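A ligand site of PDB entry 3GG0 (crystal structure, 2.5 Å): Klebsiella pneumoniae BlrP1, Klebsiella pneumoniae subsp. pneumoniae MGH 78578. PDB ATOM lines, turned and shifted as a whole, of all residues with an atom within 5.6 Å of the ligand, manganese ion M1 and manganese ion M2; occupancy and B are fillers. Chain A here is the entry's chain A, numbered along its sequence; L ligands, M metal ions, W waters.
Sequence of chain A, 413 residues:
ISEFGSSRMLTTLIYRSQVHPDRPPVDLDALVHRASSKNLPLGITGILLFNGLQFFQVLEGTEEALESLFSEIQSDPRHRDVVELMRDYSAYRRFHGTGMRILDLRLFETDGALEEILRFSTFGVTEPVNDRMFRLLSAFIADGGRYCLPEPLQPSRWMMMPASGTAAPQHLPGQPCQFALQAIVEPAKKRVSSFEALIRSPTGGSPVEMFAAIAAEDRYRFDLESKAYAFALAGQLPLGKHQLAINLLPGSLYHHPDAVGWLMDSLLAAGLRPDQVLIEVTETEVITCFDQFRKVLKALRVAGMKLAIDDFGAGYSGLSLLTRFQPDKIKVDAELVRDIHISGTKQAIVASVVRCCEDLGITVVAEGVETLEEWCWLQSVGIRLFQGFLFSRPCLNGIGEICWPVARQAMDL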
ATOM      1  N   PHE A 179     -11.861 -14.073   0.268  1.00  0.00           N
ATOM      2  CA  PHE A 179     -12.082 -15.158  -0.670  1.00  0.00           C
ATOM      3  C   PHE A 179     -11.286 -14.971  -1.944  1.00  0.00           C
ATOM      4  O   PHE A 179     -11.067 -13.846  -2.401  1.00  0.00           O
ATOM      5  CB  PHE A 179     -13.568 -15.295  -0.984  1.00  0.00           C
ATOM      6  CG  PHE A 179     -14.368 -15.927   0.119  1.00  0.00           C
ATOM      7  CD1 PHE A 179     -14.756 -15.190   1.243  1.00  0.00           C
ATOM      8  CD2 PHE A 179     -14.720 -17.275   0.061  1.00  0.00           C
ATOM      9  CE1 PHE A 179     -15.484 -15.781   2.263  1.00  0.00           C
ATOM     10  CE2 PHE A 179     -15.457 -17.870   1.070  1.00  0.00           C
ATOM     11  CZ  PHE A 179     -15.835 -17.124   2.183  1.00  0.00           C
ATOM     12  N   GLN A 182     -12.213 -18.737  -8.392  1.00  0.00           N
ATOM     13  CA  GLN A 182     -11.785 -19.516  -9.541  1.00  0.00           C
ATOM     14  C   GLN A 182     -12.915 -19.669 -10.540  1.00  0.00           C
ATOM     15  O   GLN A 182     -14.044 -20.006 -10.171  1.00  0.00           O
ATOM     16  CB  GLN A 182     -11.272 -20.890  -9.105  1.00  0.00           C
ATOM     17  CG  GLN A 182     -10.600 -21.670 -10.240  1.00  0.00           C
ATOM     18  CD  GLN A 182     -10.009 -22.982  -9.777  1.00  0.00           C
ATOM     19  OE1 GLN A 182     -10.382 -23.521  -8.729  1.00  0.00           O
ATOM     20  NE2 GLN A 182      -9.088 -23.523 -10.561  1.00  0.00           N
ATOM     21  N   GLU A 196     -16.156 -19.999  -8.437  1.00  0.00           N
ATOM     22  CA  GLU A 196     -16.191 -20.585  -7.099  1.00  0.00           C
ATOM     23  C   GLU A 196     -15.436 -19.709  -6.116  1.00  0.00           C
ATOM     24  O   GLU A 196     -14.297 -19.327  -6.360  1.00  0.00           O
ATOM     25  CB  GLU A 196     -15.607 -22.003  -7.100  1.00  0.00           C
ATOM     26  CG  GLU A 196     -15.992 -22.811  -5.841  1.00  0.00           C
ATOM     27  CD  GLU A 196     -15.261 -24.144  -5.727  1.00  0.00           C
ATOM     28  OE1 GLU A 196     -14.677 -24.620  -6.732  1.00  0.00           O
ATOM     29  OE2 GLU A 196     -15.276 -24.716  -4.619  1.00  0.00           O
ATOM     30  N   ALA A 197     -16.095 -19.384  -5.002  1.00  0.00           N
ATOM     31  CA  ALA A 197     -15.465 -18.667  -3.914  1.00  0.00           C
ATOM     32  C   ALA A 197     -14.736 -19.635  -2.996  1.00  0.00           C
ATOM     33  O   ALA A 197     -15.332 -20.604  -2.518  1.00  0.00           O
ATOM     34  CB  ALA A 197     -16.491 -17.874  -3.145  1.00  0.00           C
ATOM     35  N   LEU A 198     -13.460 -19.372  -2.754  1.00  0.00           N
ATOM     36  CA  LEU A 198     -12.631 -20.230  -1.911  1.00  0.00           C
ATOM     37  C   LEU A 198     -12.033 -19.419  -0.768  1.00  0.00           C
ATOM     38  O   LEU A 198     -11.286 -18.463  -0.992  1.00  0.00           O
ATOM     39  CB  LEU A 198     -11.515 -20.868  -2.737  1.00  0.00           C
ATOM     40  CG  LEU A 198     -11.936 -21.720  -3.938  1.00  0.00           C
ATOM     41  CD1 LEU A 198     -10.770 -21.944  -4.891  1.00  0.00           C
ATOM     42  CD2 LEU A 198     -12.538 -23.032  -3.490  1.00  0.00           C
ATOM     43  N   ILE A 199     -12.360 -19.806   0.467  1.00  0.00           N
ATOM     44  CA  ILE A 199     -12.007 -19.021   1.654  1.00  0.00           C
ATOM     45  C   ILE A 199     -10.488 -18.904   1.875  1.00  0.00           C
ATOM     46  O   ILE A 199      -9.735 -19.868   1.713  1.00  0.00           O
ATOM     47  CB  ILE A 199     -12.705 -19.572   2.919  1.00  0.00           C
ATOM     48  CG1 ILE A 199     -12.721 -18.510   4.026  1.00  0.00           C
ATOM     49  CG2 ILE A 199     -12.058 -20.862   3.395  1.00  0.00           C
ATOM     50  CD1 ILE A 199     -13.643 -18.842   5.183  1.00  0.00           C
ATOM     51  N   ARG A 200     -10.046 -17.697   2.210  1.00  0.00           N
ATOM     52  CA  ARG A 200      -8.654 -17.450   2.557  1.00  0.00           C
ATOM     53  C   ARG A 200      -8.546 -16.746   3.895  1.00  0.00           C
ATOM     54  O   ARG A 200      -9.440 -15.973   4.282  1.00  0.00           O
ATOM     55  CB  ARG A 200      -7.964 -16.611   1.469  1.00  0.00           C
ATOM     56  CG  ARG A 200      -7.978 -17.243   0.074  1.00  0.00           C
ATOM     57  CD  ARG A 200      -6.957 -18.360  -0.032  1.00  0.00           C
ATOM     58  NE  ARG A 200      -6.923 -18.947  -1.369  1.00  0.00           N
ATOM     59  CZ  ARG A 200      -7.681 -19.973  -1.743  1.00  0.00           C
ATOM     60  NH1 ARG A 200      -8.540 -20.536  -0.894  1.00  0.00           N
ATOM     61  NH2 ARG A 200      -7.584 -20.451  -2.983  1.00  0.00           N
ATOM     62  N   SER A 206      -4.339 -20.424   3.417  1.00  0.00           N
ATOM     63  CA  SER A 206      -5.234 -21.483   2.959  1.00  0.00           C
ATOM     64  C   SER A 206      -6.512 -21.599   3.803  1.00  0.00           C
ATOM     65  O   SER A 206      -6.562 -21.085   4.916  1.00  0.00           O
ATOM     66  CB  SER A 206      -4.490 -22.826   2.952  1.00  0.00           C
ATOM     67  OG  SER A 206      -4.367 -23.357   4.246  1.00  0.00           O
ATOM     68  N   PRO A 207      -7.554 -22.255   3.255  1.00  0.00           N
ATOM     69  CA  PRO A 207      -8.755 -22.632   4.019  1.00  0.00           C
ATOM     70  C   PRO A 207      -8.429 -23.299   5.355  1.00  0.00           C
ATOM     71  O   PRO A 207      -9.066 -22.986   6.372  1.00  0.00           O
ATOM     72  CB  PRO A 207      -9.452 -23.632   3.085  1.00  0.00           C
ATOM     73  CG  PRO A 207      -9.074 -23.177   1.726  1.00  0.00           C
ATOM     74  CD  PRO A 207      -7.671 -22.637   1.834  1.00  0.00           C
ATOM     75  N   PHE A 211      -9.476 -21.876   9.116  1.00  0.00           N
ATOM     76  CA  PHE A 211     -10.300 -22.588  10.091  1.00  0.00           C
ATOM     77  C   PHE A 211      -9.522 -22.998  11.345  1.00  0.00           C
ATOM     78  O   PHE A 211     -10.116 -23.169  12.405  1.00  0.00           O
ATOM     79  CB  PHE A 211     -10.976 -23.801   9.442  1.00  0.00           C
ATOM     80  CG  PHE A 211     -12.239 -23.468   8.689  1.00  0.00           C
ATOM     81  CD1 PHE A 211     -13.431 -23.229   9.363  1.00  0.00           C
ATOM     82  CD2 PHE A 211     -12.229 -23.383   7.296  1.00  0.00           C
ATOM     83  CE1 PHE A 211     -14.584 -22.914   8.672  1.00  0.00           C
ATOM     84  CE2 PHE A 211     -13.381 -23.070   6.595  1.00  0.00           C
ATOM     85  CZ  PHE A 211     -14.564 -22.837   7.282  1.00  0.00           C
ATOM     86  N   ASP A 223     -18.117 -20.777   9.183  1.00  0.00           N
ATOM     87  CA  ASP A 223     -18.266 -21.228   7.797  1.00  0.00           C
ATOM     88  C   ASP A 223     -19.493 -20.588   7.149  1.00  0.00           C
ATOM     89  O   ASP A 223     -19.428 -20.109   6.020  1.00  0.00           O
ATOM     90  CB  ASP A 223     -18.370 -22.759   7.736  1.00  0.00           C
ATOM     91  CG  ASP A 223     -18.450 -23.292   6.317  1.00  0.00           C
ATOM     92  OD1 ASP A 223     -17.928 -22.633   5.396  1.00  0.00           O
ATOM     93  OD2 ASP A 223     -19.030 -24.378   6.119  1.00  0.00           O
ATOM     94  N   SER A 226     -19.006 -16.509   7.120  1.00  0.00           N
ATOM     95  CA  SER A 226     -18.017 -16.023   6.142  1.00  0.00           C
ATOM     96  C   SER A 226     -18.584 -15.852   4.739  1.00  0.00           C
ATOM     97  O   SER A 226     -18.069 -15.061   3.961  1.00  0.00           O
ATOM     98  CB  SER A 226     -16.795 -16.943   6.110  1.00  0.00           C
ATOM     99  OG  SER A 226     -17.153 -18.268   5.753  1.00  0.00           O
ATOM    100  N   LYS A 227     -19.660 -16.571   4.441  1.00  0.00           N
ATOM    101  CA  LYS A 227     -20.288 -16.501   3.126  1.00  0.00           C
ATOM    102  C   LYS A 227     -20.803 -15.114   2.780  1.00  0.00           C
ATOM    103  O   LYS A 227     -20.923 -14.770   1.605  1.00  0.00           O
ATOM    104  CB  LYS A 227     -21.430 -17.531   3.031  1.00  0.00           C
ATOM    105  CG  LYS A 227     -20.953 -18.969   3.020  1.00  0.00           C
ATOM    106  CD  LYS A 227     -19.650 -19.098   2.261  1.00  0.00           C
ATOM    107  CE  LYS A 227     -19.141 -20.502   2.278  1.00  0.00           C
ATOM    108  NZ  LYS A 227     -18.340 -20.792   3.495  1.00  0.00           N
ATOM    109  N   ASN A 247     -18.802 -23.180  -0.992  1.00  0.00           N
ATOM    110  CA  ASN A 247     -18.594 -24.405  -0.221  1.00  0.00           C
ATOM    111  C   ASN A 247     -19.125 -24.280   1.201  1.00  0.00           C
ATOM    112  O   ASN A 247     -18.657 -23.452   1.978  1.00  0.00           O
ATOM    113  CB  ASN A 247     -17.103 -24.770  -0.176  1.00  0.00           C
ATOM    114  CG  ASN A 247     -16.495 -24.954  -1.552  1.00  0.00           C
ATOM    115  OD1 ASN A 247     -16.444 -26.073  -2.077  1.00  0.00           O
ATOM    116  ND2 ASN A 247     -16.015 -23.853  -2.131  1.00  0.00           N
ATOM    117  N   LEU A 248     -20.119 -25.071   1.557  1.00  0.00           N
ATOM    118  CA  LEU A 248     -20.574 -25.175   2.943  1.00  0.00           C
ATOM    119  C   LEU A 248     -20.580 -26.624   3.396  1.00  0.00           C
ATOM    120  O   LEU A 248     -21.042 -27.502   2.663  1.00  0.00           O
ATOM    121  CB  LEU A 248     -21.966 -24.569   3.112  1.00  0.00           C
ATOM    122  CG  LEU A 248     -22.092 -23.054   3.248  1.00  0.00           C
ATOM    123  CD1 LEU A 248     -23.566 -22.648   3.268  1.00  0.00           C
ATOM    124  CD2 LEU A 248     -21.385 -22.557   4.485  1.00  0.00           C
ATOM    125  N   LEU A 249     -20.070 -26.871   4.592  1.00  0.00           N
ATOM    126  CA  LEU A 249     -20.295 -28.136   5.269  1.00  0.00           C
ATOM    127  C   LEU A 249     -21.761 -28.220   5.683  1.00  0.00           C
ATOM    128  O   LEU A 249     -22.350 -27.210   6.076  1.00  0.00           O
ATOM    129  CB  LEU A 249     -19.381 -28.270   6.495  1.00  0.00           C
ATOM    130  CG  LEU A 249     -17.886 -28.050   6.260  1.00  0.00           C
ATOM    131  CD1 LEU A 249     -17.098 -28.150   7.563  1.00  0.00           C
ATOM    132  CD2 LEU A 249     -17.332 -29.021   5.218  1.00  0.00           C
ATOM    133  N   GLU A 280     -22.045 -25.728  -2.666  1.00  0.00           N
ATOM    134  CA  GLU A 280     -21.236 -26.925  -2.866  1.00  0.00           C
ATOM    135  C   GLU A 280     -21.073 -27.687  -1.560  1.00  0.00           C
ATOM    136  O   GLU A 280     -20.469 -27.199  -0.607  1.00  0.00           O
ATOM    137  CB  GLU A 280     -19.861 -26.554  -3.406  1.00  0.00           C
ATOM    138  CG  GLU A 280     -19.854 -26.049  -4.831  1.00  0.00           C
ATOM    139  CD  GLU A 280     -18.460 -25.934  -5.398  1.00  0.00           C
ATOM    140  OE1 GLU A 280     -18.290 -25.244  -6.430  1.00  0.00           O
ATOM    141  OE2 GLU A 280     -17.528 -26.537  -4.833  1.00  0.00           O
ATOM    142  N   THR A 282     -19.665 -31.427   0.071  1.00  0.00           N
ATOM    143  CA  THR A 282     -18.787 -32.563  -0.217  1.00  0.00           C
ATOM    144  C   THR A 282     -19.525 -33.890  -0.129  1.00  0.00           C
ATOM    145  O   THR A 282     -20.329 -34.114   0.779  1.00  0.00           O
ATOM    146  CB  THR A 282     -17.553 -32.606   0.699  1.00  0.00           C
ATOM    147  OG1 THR A 282     -17.896 -32.090   1.988  1.00  0.00           O
ATOM    148  CG2 THR A 282     -16.429 -31.783   0.115  1.00  0.00           C
ATOM    149  N   ASP A 310     -19.961 -31.527  -4.420  1.00  0.00           N
ATOM    150  CA  ASP A 310     -18.553 -31.285  -4.642  1.00  0.00           C
ATOM    151  C   ASP A 310     -17.746 -32.559  -4.470  1.00  0.00           C
ATOM    152  O   ASP A 310     -18.090 -33.417  -3.650  1.00  0.00           O
ATOM    153  CB  ASP A 310     -18.046 -30.206  -3.694  1.00  0.00           C
ATOM    154  CG  ASP A 310     -16.745 -29.579  -4.172  1.00  0.00           C
ATOM    155  OD1 ASP A 310     -16.303 -29.879  -5.303  1.00  0.00           O
ATOM    156  OD2 ASP A 310     -16.181 -28.771  -3.408  1.00  0.00           O
ATOM    157  N   ASP A 311     -16.676 -32.689  -5.251  1.00  0.00           N
ATOM    158  CA  ASP A 311     -15.744 -33.826  -5.147  1.00  0.00           C
ATOM    159  C   ASP A 311     -16.433 -35.187  -5.292  1.00  0.00           C
ATOM    160  O   ASP A 311     -16.153 -36.124  -4.540  1.00  0.00           O
ATOM    161  CB  ASP A 311     -14.938 -33.746  -3.844  1.00  0.00           C
ATOM    162  CG  ASP A 311     -14.046 -32.502  -3.786  1.00  0.00           C
ATOM    163  OD1 ASP A 311     -13.811 -31.873  -4.845  1.00  0.00           O
ATOM    164  OD2 ASP A 311     -13.574 -32.161  -2.679  1.00  0.00           O
ATOM    165  N   LYS A 331     -19.619 -32.139  -9.463  1.00  0.00           N
ATOM    166  CA  LYS A 331     -18.219 -31.820  -9.747  1.00  0.00           C
ATOM    167  C   LYS A 331     -17.355 -33.053  -9.607  1.00  0.00           C
ATOM    168  O   LYS A 331     -17.101 -33.532  -8.505  1.00  0.00           O
ATOM    169  CB  LYS A 331     -17.714 -30.703  -8.849  1.00  0.00           C
ATOM    170  CG  LYS A 331     -18.554 -29.430  -8.891  1.00  0.00           C
ATOM    171  CD  LYS A 331     -18.000 -28.363  -7.974  1.00  0.00           C
ATOM    172  CE  LYS A 331     -17.051 -27.461  -8.707  1.00  0.00           C
ATOM    173  NZ  LYS A 331     -16.228 -26.650  -7.771  1.00  0.00           N
ATOM    174  N   ARG A 338      -6.895 -36.744 -12.899  1.00  0.00           N
ATOM    175  CA  ARG A 338      -5.468 -37.092 -12.951  1.00  0.00           C
ATOM    176  C   ARG A 338      -5.246 -38.298 -13.815  1.00  0.00           C
ATOM    177  O   ARG A 338      -5.752 -39.384 -13.514  1.00  0.00           O
ATOM    178  CB  ARG A 338      -4.920 -37.382 -11.551  1.00  0.00           C
ATOM    179  CG  ARG A 338      -4.640 -36.171 -10.720  1.00  0.00           C
ATOM    180  CD  ARG A 338      -3.592 -35.247 -11.350  1.00  0.00           C
ATOM    181  NE  ARG A 338      -3.747 -33.899 -10.813  1.00  0.00           N
ATOM    182  CZ  ARG A 338      -4.559 -32.978 -11.315  1.00  0.00           C
ATOM    183  NH1 ARG A 338      -5.262 -33.237 -12.413  1.00  0.00           N
ATOM    184  NH2 ARG A 338      -4.668 -31.799 -10.729  1.00  0.00           N
ATOM    185  N   GLU A 367     -12.892 -31.310 -12.417  1.00  0.00           N
ATOM    186  CA  GLU A 367     -12.075 -30.508 -11.511  1.00  0.00           C
ATOM    187  C   GLU A 367     -10.614 -30.846 -11.622  1.00  0.00           C
ATOM    188  O   GLU A 367     -10.253 -31.944 -12.015  1.00  0.00           O
ATOM    189  CB  GLU A 367     -12.509 -30.745 -10.089  1.00  0.00           C
ATOM    190  CG  GLU A 367     -13.344 -29.677  -9.496  1.00  0.00           C
ATOM    191  CD  GLU A 367     -13.632 -29.939  -8.057  1.00  0.00           C
ATOM    192  OE1 GLU A 367     -13.162 -29.171  -7.192  1.00  0.00           O
ATOM    193  OE2 GLU A 367     -14.291 -30.960  -7.773  1.00  0.00           O
ATOM    194  N   GLY A 368      -9.764 -29.895 -11.227  1.00  0.00           N
ATOM    195  CA  GLY A 368      -8.331 -30.124 -11.152  1.00  0.00           C
ATOM    196  C   GLY A 368      -7.698 -30.402 -12.500  1.00  0.00           C
ATOM    197  O   GLY A 368      -6.687 -31.094 -12.578  1.00  0.00           O
ATOM    198  N   VAL A 369      -8.284 -29.858 -13.562  1.00  0.00           N
ATOM    199  CA  VAL A 369      -7.738 -29.994 -14.917  1.00  0.00           C
ATOM    200  C   VAL A 369      -6.477 -29.144 -15.093  1.00  0.00           C
ATOM    201  O   VAL A 369      -6.531 -27.914 -15.043  1.00  0.00           O
ATOM    202  CB  VAL A 369      -8.775 -29.609 -15.994  1.00  0.00           C
ATOM    203  CG1 VAL A 369      -8.227 -29.900 -17.383  1.00  0.00           C
ATOM    204  CG2 VAL A 369     -10.080 -30.357 -15.767  1.00  0.00           C
ATOM    205  N   GLU A 370      -5.345 -29.810 -15.296  1.00  0.00           N
ATOM    206  CA  GLU A 370      -4.049 -29.128 -15.300  1.00  0.00           C
ATOM    207  C   GLU A 370      -3.344 -29.186 -16.651  1.00  0.00           C
ATOM    208  O   GLU A 370      -2.453 -28.377 -16.922  1.00  0.00           O
ATOM    209  CB  GLU A 370      -3.138 -29.723 -14.230  1.00  0.00           C
ATOM    210  CG  GLU A 370      -3.502 -29.332 -12.809  1.00  0.00           C
ATOM    211  CD  GLU A 370      -2.602 -30.004 -11.784  1.00  0.00           C
ATOM    212  OE1 GLU A 370      -1.958 -31.004 -12.129  1.00  0.00           O
ATOM    213  OE2 GLU A 370      -2.568 -29.529 -10.628  1.00  0.00           O
ATOM    214  N   GLN A 387     -12.921 -26.916 -14.627  1.00  0.00           N
ATOM    215  CA  GLN A 387     -12.314 -26.093 -13.600  1.00  0.00           C
ATOM    216  C   GLN A 387     -10.913 -26.602 -13.303  1.00  0.00           C
ATOM    217  O   GLN A 387     -10.731 -27.777 -12.985  1.00  0.00           O
ATOM    218  CB  GLN A 387     -13.162 -26.109 -12.324  1.00  0.00           C
ATOM    219  CG  GLN A 387     -12.575 -25.305 -11.160  1.00  0.00           C
ATOM    220  CD  GLN A 387     -13.502 -25.238  -9.957  1.00  0.00           C
ATOM    221  OE1 GLN A 387     -14.521 -25.903  -9.896  1.00  0.00           O
ATOM    222  NE2 GLN A 387     -13.143 -24.426  -8.984  1.00  0.00           N
ATOM    223  N   GLY A 388      -9.916 -25.735 -13.418  1.00  0.00           N
ATOM    224  CA  GLY A 388      -8.548 -26.122 -13.114  1.00  0.00           C
ATOM    225  C   GLY A 388      -7.494 -25.082 -13.398  1.00  0.00           C
ATOM    226  O   GLY A 388      -7.767 -24.066 -14.055  1.00  0.00           O
ATOM    227  N   PHE A 389      -6.280 -25.338 -12.911  1.00  0.00           N
ATOM    228  CA  PHE A 389      -5.159 -24.407 -13.054  1.00  0.00           C
ATOM    229  C   PHE A 389      -4.782 -24.168 -14.516  1.00  0.00           C
ATOM    230  O   PHE A 389      -4.192 -23.139 -14.843  1.00  0.00           O
ATOM    231  CB  PHE A 389      -3.935 -24.922 -12.292  1.00  0.00           C
ATOM    232  CG  PHE A 389      -4.064 -24.852 -10.799  1.00  0.00           C
ATOM    233  CD1 PHE A 389      -5.066 -24.102 -10.203  1.00  0.00           C
ATOM    234  CD2 PHE A 389      -3.164 -25.528  -9.981  1.00  0.00           C
ATOM    235  CE1 PHE A 389      -5.186 -24.027  -8.814  1.00  0.00           C
ATOM    236  CE2 PHE A 389      -3.265 -25.449  -8.590  1.00  0.00           C
ATOM    237  CZ  PHE A 389      -4.283 -24.708  -8.016  1.00  0.00           C
ATOM    238  N   LEU A 390      -5.125 -25.128 -15.388  1.00  0.00           N
ATOM    239  CA  LEU A 390      -4.909 -24.980 -16.819  1.00  0.00           C
ATOM    240  C   LEU A 390      -5.637 -23.765 -17.371  1.00  0.00           C
ATOM    241  O   LEU A 390      -5.067 -22.996 -18.146  1.00  0.00           O
ATOM    242  CB  LEU A 390      -5.353 -26.234 -17.559  1.00  0.00           C
ATOM    243  CG  LEU A 390      -5.153 -26.228 -19.082  1.00  0.00           C
ATOM    244  CD1 LEU A 390      -3.679 -26.391 -19.444  1.00  0.00           C
ATOM    245  CD2 LEU A 390      -5.995 -27.303 -19.747  1.00  0.00           C
ATOM    246  N   SER A 392      -7.648 -21.415 -15.280  1.00  0.00           N
ATOM    247  CA  SER A 392      -7.809 -20.291 -14.365  1.00  0.00           C
ATOM    248  C   SER A 392      -7.383 -20.650 -12.955  1.00  0.00           C
ATOM    249  O   SER A 392      -7.830 -21.644 -12.387  1.00  0.00           O
ATOM    250  CB  SER A 392      -9.273 -19.825 -14.358  1.00  0.00           C
ATOM    251  OG  SER A 392      -9.493 -18.795 -13.408  1.00  0.00           O
ATOM    252  N   PRO A 394      -7.133 -19.603  -8.810  1.00  0.00           N
ATOM    253  CA  PRO A 394      -7.729 -18.811  -7.751  1.00  0.00           C
ATOM    254  C   PRO A 394      -7.110 -17.434  -7.661  1.00  0.00           C
ATOM    255  O   PRO A 394      -5.880 -17.301  -7.642  1.00  0.00           O
ATOM    256  CB  PRO A 394      -7.400 -19.614  -6.494  1.00  0.00           C
ATOM    257  CG  PRO A 394      -7.367 -21.011  -6.954  1.00  0.00           C
ATOM    258  CD  PRO A 394      -6.836 -20.976  -8.364  1.00  0.00           C
HETATM  259  P1  LIG L   1     -12.670 -27.704  -3.179  1.00  0.00           P
HETATM  260  O1  LIG L   1     -13.664 -26.588  -3.017  1.00  0.00           O
HETATM  261  O2  LIG L   1     -13.428 -29.009  -3.234  1.00  0.00           O
HETATM  262  O3  LIG L   1     -11.877 -27.495  -4.564  1.00  0.00           O
HETATM  263  C1  LIG L   1     -11.164 -26.279  -4.816  1.00  0.00           C
HETATM  264  C2  LIG L   1      -9.692 -26.479  -4.461  1.00  0.00           C
HETATM  265  O4  LIG L   1      -9.020 -27.127  -5.535  1.00  0.00           O
HETATM  266  C3  LIG L   1      -8.976 -25.150  -4.335  1.00  0.00           C
HETATM  267  O5  LIG L   1      -7.979 -25.287  -3.325  1.00  0.00           O
HETATM  268  C4  LIG L   1      -8.282 -25.000  -5.646  1.00  0.00           C
HETATM  269  O6  LIG L   1      -7.198 -24.240  -5.512  1.00  0.00           O
HETATM  270  C5  LIG L   1      -7.950 -26.248  -5.995  1.00  0.00           C
HETATM  271  N1  LIG L   1      -7.740 -26.392  -7.344  1.00  0.00           N
HETATM  272  C6  LIG L   1      -8.454 -25.847  -8.248  1.00  0.00           C
HETATM  273  N2  LIG L   1      -7.973 -26.188  -9.395  1.00  0.00           N
HETATM  274  C7  LIG L   1      -6.902 -26.995  -9.238  1.00  0.00           C
HETATM  275  C8  LIG L   1      -6.006 -27.643 -10.092  1.00  0.00           C
HETATM  276  O7  LIG L   1      -6.114 -27.557 -11.336  1.00  0.00           O
HETATM  277  N3  LIG L   1      -5.025 -28.391  -9.547  1.00  0.00           N
HETATM  278  C9  LIG L   1      -4.892 -28.508  -8.198  1.00  0.00           C
HETATM  279  N4  LIG L   1      -3.894 -29.266  -7.700  1.00  0.00           N
HETATM  280  N5  LIG L   1      -5.753 -27.878  -7.355  1.00  0.00           N
HETATM  281  C10 LIG L   1      -6.748 -27.132  -7.860  1.00  0.00           C
HETATM  282  P2  LIG L   1      -8.390 -24.551  -1.955  1.00  0.00           P
HETATM  283  O8  LIG L   1      -7.069 -24.087  -1.193  1.00  0.00           O
HETATM  284  O9  LIG L   1      -9.237 -23.227  -2.229  1.00  0.00           O
HETATM  285  O10 LIG L   1      -9.499 -25.399  -1.164  1.00  0.00           O
HETATM  286  C11 LIG L   1      -9.202 -26.385  -0.179  1.00  0.00           C
HETATM  287  C12 LIG L   1     -10.631 -26.862   0.077  1.00  0.00           C
HETATM  288  O11 LIG L   1     -11.218 -26.141   1.177  1.00  0.00           O
HETATM  289  C13 LIG L   1     -11.595 -26.657  -1.090  1.00  0.00           C
HETATM  290  O12 LIG L   1     -11.620 -27.803  -1.943  1.00  0.00           O
HETATM  291  C14 LIG L   1     -12.898 -26.454  -0.370  1.00  0.00           C
HETATM  292  O13 LIG L   1     -13.330 -27.628   0.068  1.00  0.00           O
HETATM  293  C15 LIG L   1     -12.505 -25.753   0.677  1.00  0.00           C
HETATM  294  N6  LIG L   1     -13.119 -24.569   0.991  1.00  0.00           N
HETATM  295  C16 LIG L   1     -12.861 -23.473   0.288  1.00  0.00           C
HETATM  296  N7  LIG L   1     -13.676 -22.526   0.809  1.00  0.00           N
HETATM  297  C17 LIG L   1     -14.443 -23.105   1.779  1.00  0.00           C
HETATM  298  C18 LIG L   1     -15.423 -22.600   2.616  1.00  0.00           C
HETATM  299  O14 LIG L   1     -15.766 -21.406   2.540  1.00  0.00           O
HETATM  300  N8  LIG L   1     -16.022 -23.439   3.498  1.00  0.00           N
HETATM  301  C19 LIG L   1     -15.660 -24.743   3.583  1.00  0.00           C
HETATM  302  N9  LIG L   1     -16.280 -25.535   4.492  1.00  0.00           N
HETATM  303  N10 LIG L   1     -14.692 -25.251   2.777  1.00  0.00           N
HETATM  304  C20 LIG L   1     -14.087 -24.439   1.871  1.00  0.00           C
HETATM  305 MN    MN M   1     -15.731 -26.704  -4.003  1.00  0.00          MN
HETATM  306 MN    MN M   2     -13.938 -29.742  -5.414  1.00  0.00          MN
HETATM  307  O   HOH W   1     -16.411 -20.863   0.003  1.00  0.00           O
HETATM  308  O   HOH W   2      -9.129 -29.380  -7.217  1.00  0.00           O
HETATM  309  O   HOH W   3     -14.740 -27.562  -5.957  1.00  0.00           O
HETATM  310  O   HOH W   4      -4.536 -23.290  -0.279  1.00  0.00           O
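O of Asn 247 is in hydrogen-bond range of N8 of the ligand (3.0 Å).
N of Ile 199 sits at hydrogen-bond distance from N7 of the ligand (3.0 Å).
The backbone NH (N) of Phe 389 lies within hydrogen-bond range of an oxygen (O7) of the ligand.
A nitrogen (N8) of the ligand sits at hydrogen-bond distance from the side-chain carboxylate (OD1) of Asp 223.
O14 of the ligand lies within hydrogen-bond range of NZ of Lys 227 (2.8 Å).
The guanidinium group (NH1) of Arg 200 lies within salt-bridge range of an oxygen (O9) of the ligand (3.1 Å).
The side-chain amide nitrogen of Gln 182 is in hydrogen-bond range of a nitrogen (N2) of the ligand (3.1 Å).
OE2 of Glu 370 sits at hydrogen-bond distance from N3 of the ligand (2.9 Å).
The side-chain carboxylate (OD1) of Asp 223 is in salt-bridge range of the side-chain amino group (NZ) of Lys 227 (2.7 Å).
The side-chain amide nitrogen of Gln 182 sits at hydrogen-bond distance from the backbone carbonyl oxygen of Ser 392, 2.9 Å away.
O of Asn 247 lies close to NZ of Lys 227, at 3.1 Å.
The side-chain hydroxyl (OG) of Ser 226 lies within hydrogen-bond range of the backbone carbonyl oxygen (O) of Asp 223 (2.9 Å).
ND2 of Asn 247 is in hydrogen-bond range of O of Ala 197 (3.3 Å).
O of Gln 182 is in hydrogen-bond range of N of Glu 196 (2.7 Å).
OE1 of Glu 280 is in salt-bridge range of NZ of Lys 331 (2.8 Å).
OE1 of Glu 196 lies within salt-bridge range of NZ of Lys 331.
Phe 179 touches the ligand.
Leu 198 touches the ligand (CB to O9, 3.3 Å).
CD of Pro 207 touches O8 of the ligand (3.4 Å).
Leu 249 touches the ligand.
Arg 338 touches the ligand (NH2 to N3, 3.6 Å).
Gly 368 touches the ligand.
Val 369 touches the ligand (O to O7, 3.7 Å).
Gly 388 touches the ligand (CA to O7, 3.3 Å).
CG of Pro 394 touches O6 of the ligand, 3.5 Å away.
The nearest printed residue that does not touch the ligand is Phe 211 (4.1 Å).
Lys 331 touches manganese ion M1.
Of the 32 residues printed, 5 come within 4 Å of manganese ion M1.
The nearest printed residue that does not touch manganese ion M1 is Glu 367 (4.8 Å).
Of the 32 residues printed, 3 come within 4 Å of manganese ion M2.
The nearest printed residue that does not touch manganese ion M2 is Lys 331 (4.5 Å).
Manganese ion M1 is bound by OE2 of Glu 280 (2.0 Å), OE2 of Glu 196 (2.1 Å), OD1 of Asn 247 (2.1 Å), OD2 of Asp 310 (2.2 Å), O1 of the ligand (2.3 Å) and water W3 (2.4 Å).
Manganese ion M1 has six donor atoms within binding distance.
Manganese ion M2 is bound by OE1 of Glu 367, OD1 of Asp 311, O2 of the ligand, OD1 of Asp 310, water W3 and OE2 of Glu 367.
Manganese ion M2 has six donor atoms within binding distance.
Water W3 lies within hydrogen-bond range of NZ of Lys 331, OE1 of Glu 196 and O3 of the ligand.
Water W1 lies within hydrogen-bond range of O14 of the ligand (2.7 Å), O of Ala 197 (2.8 Å) and N of Asn 247 (3.5 Å).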
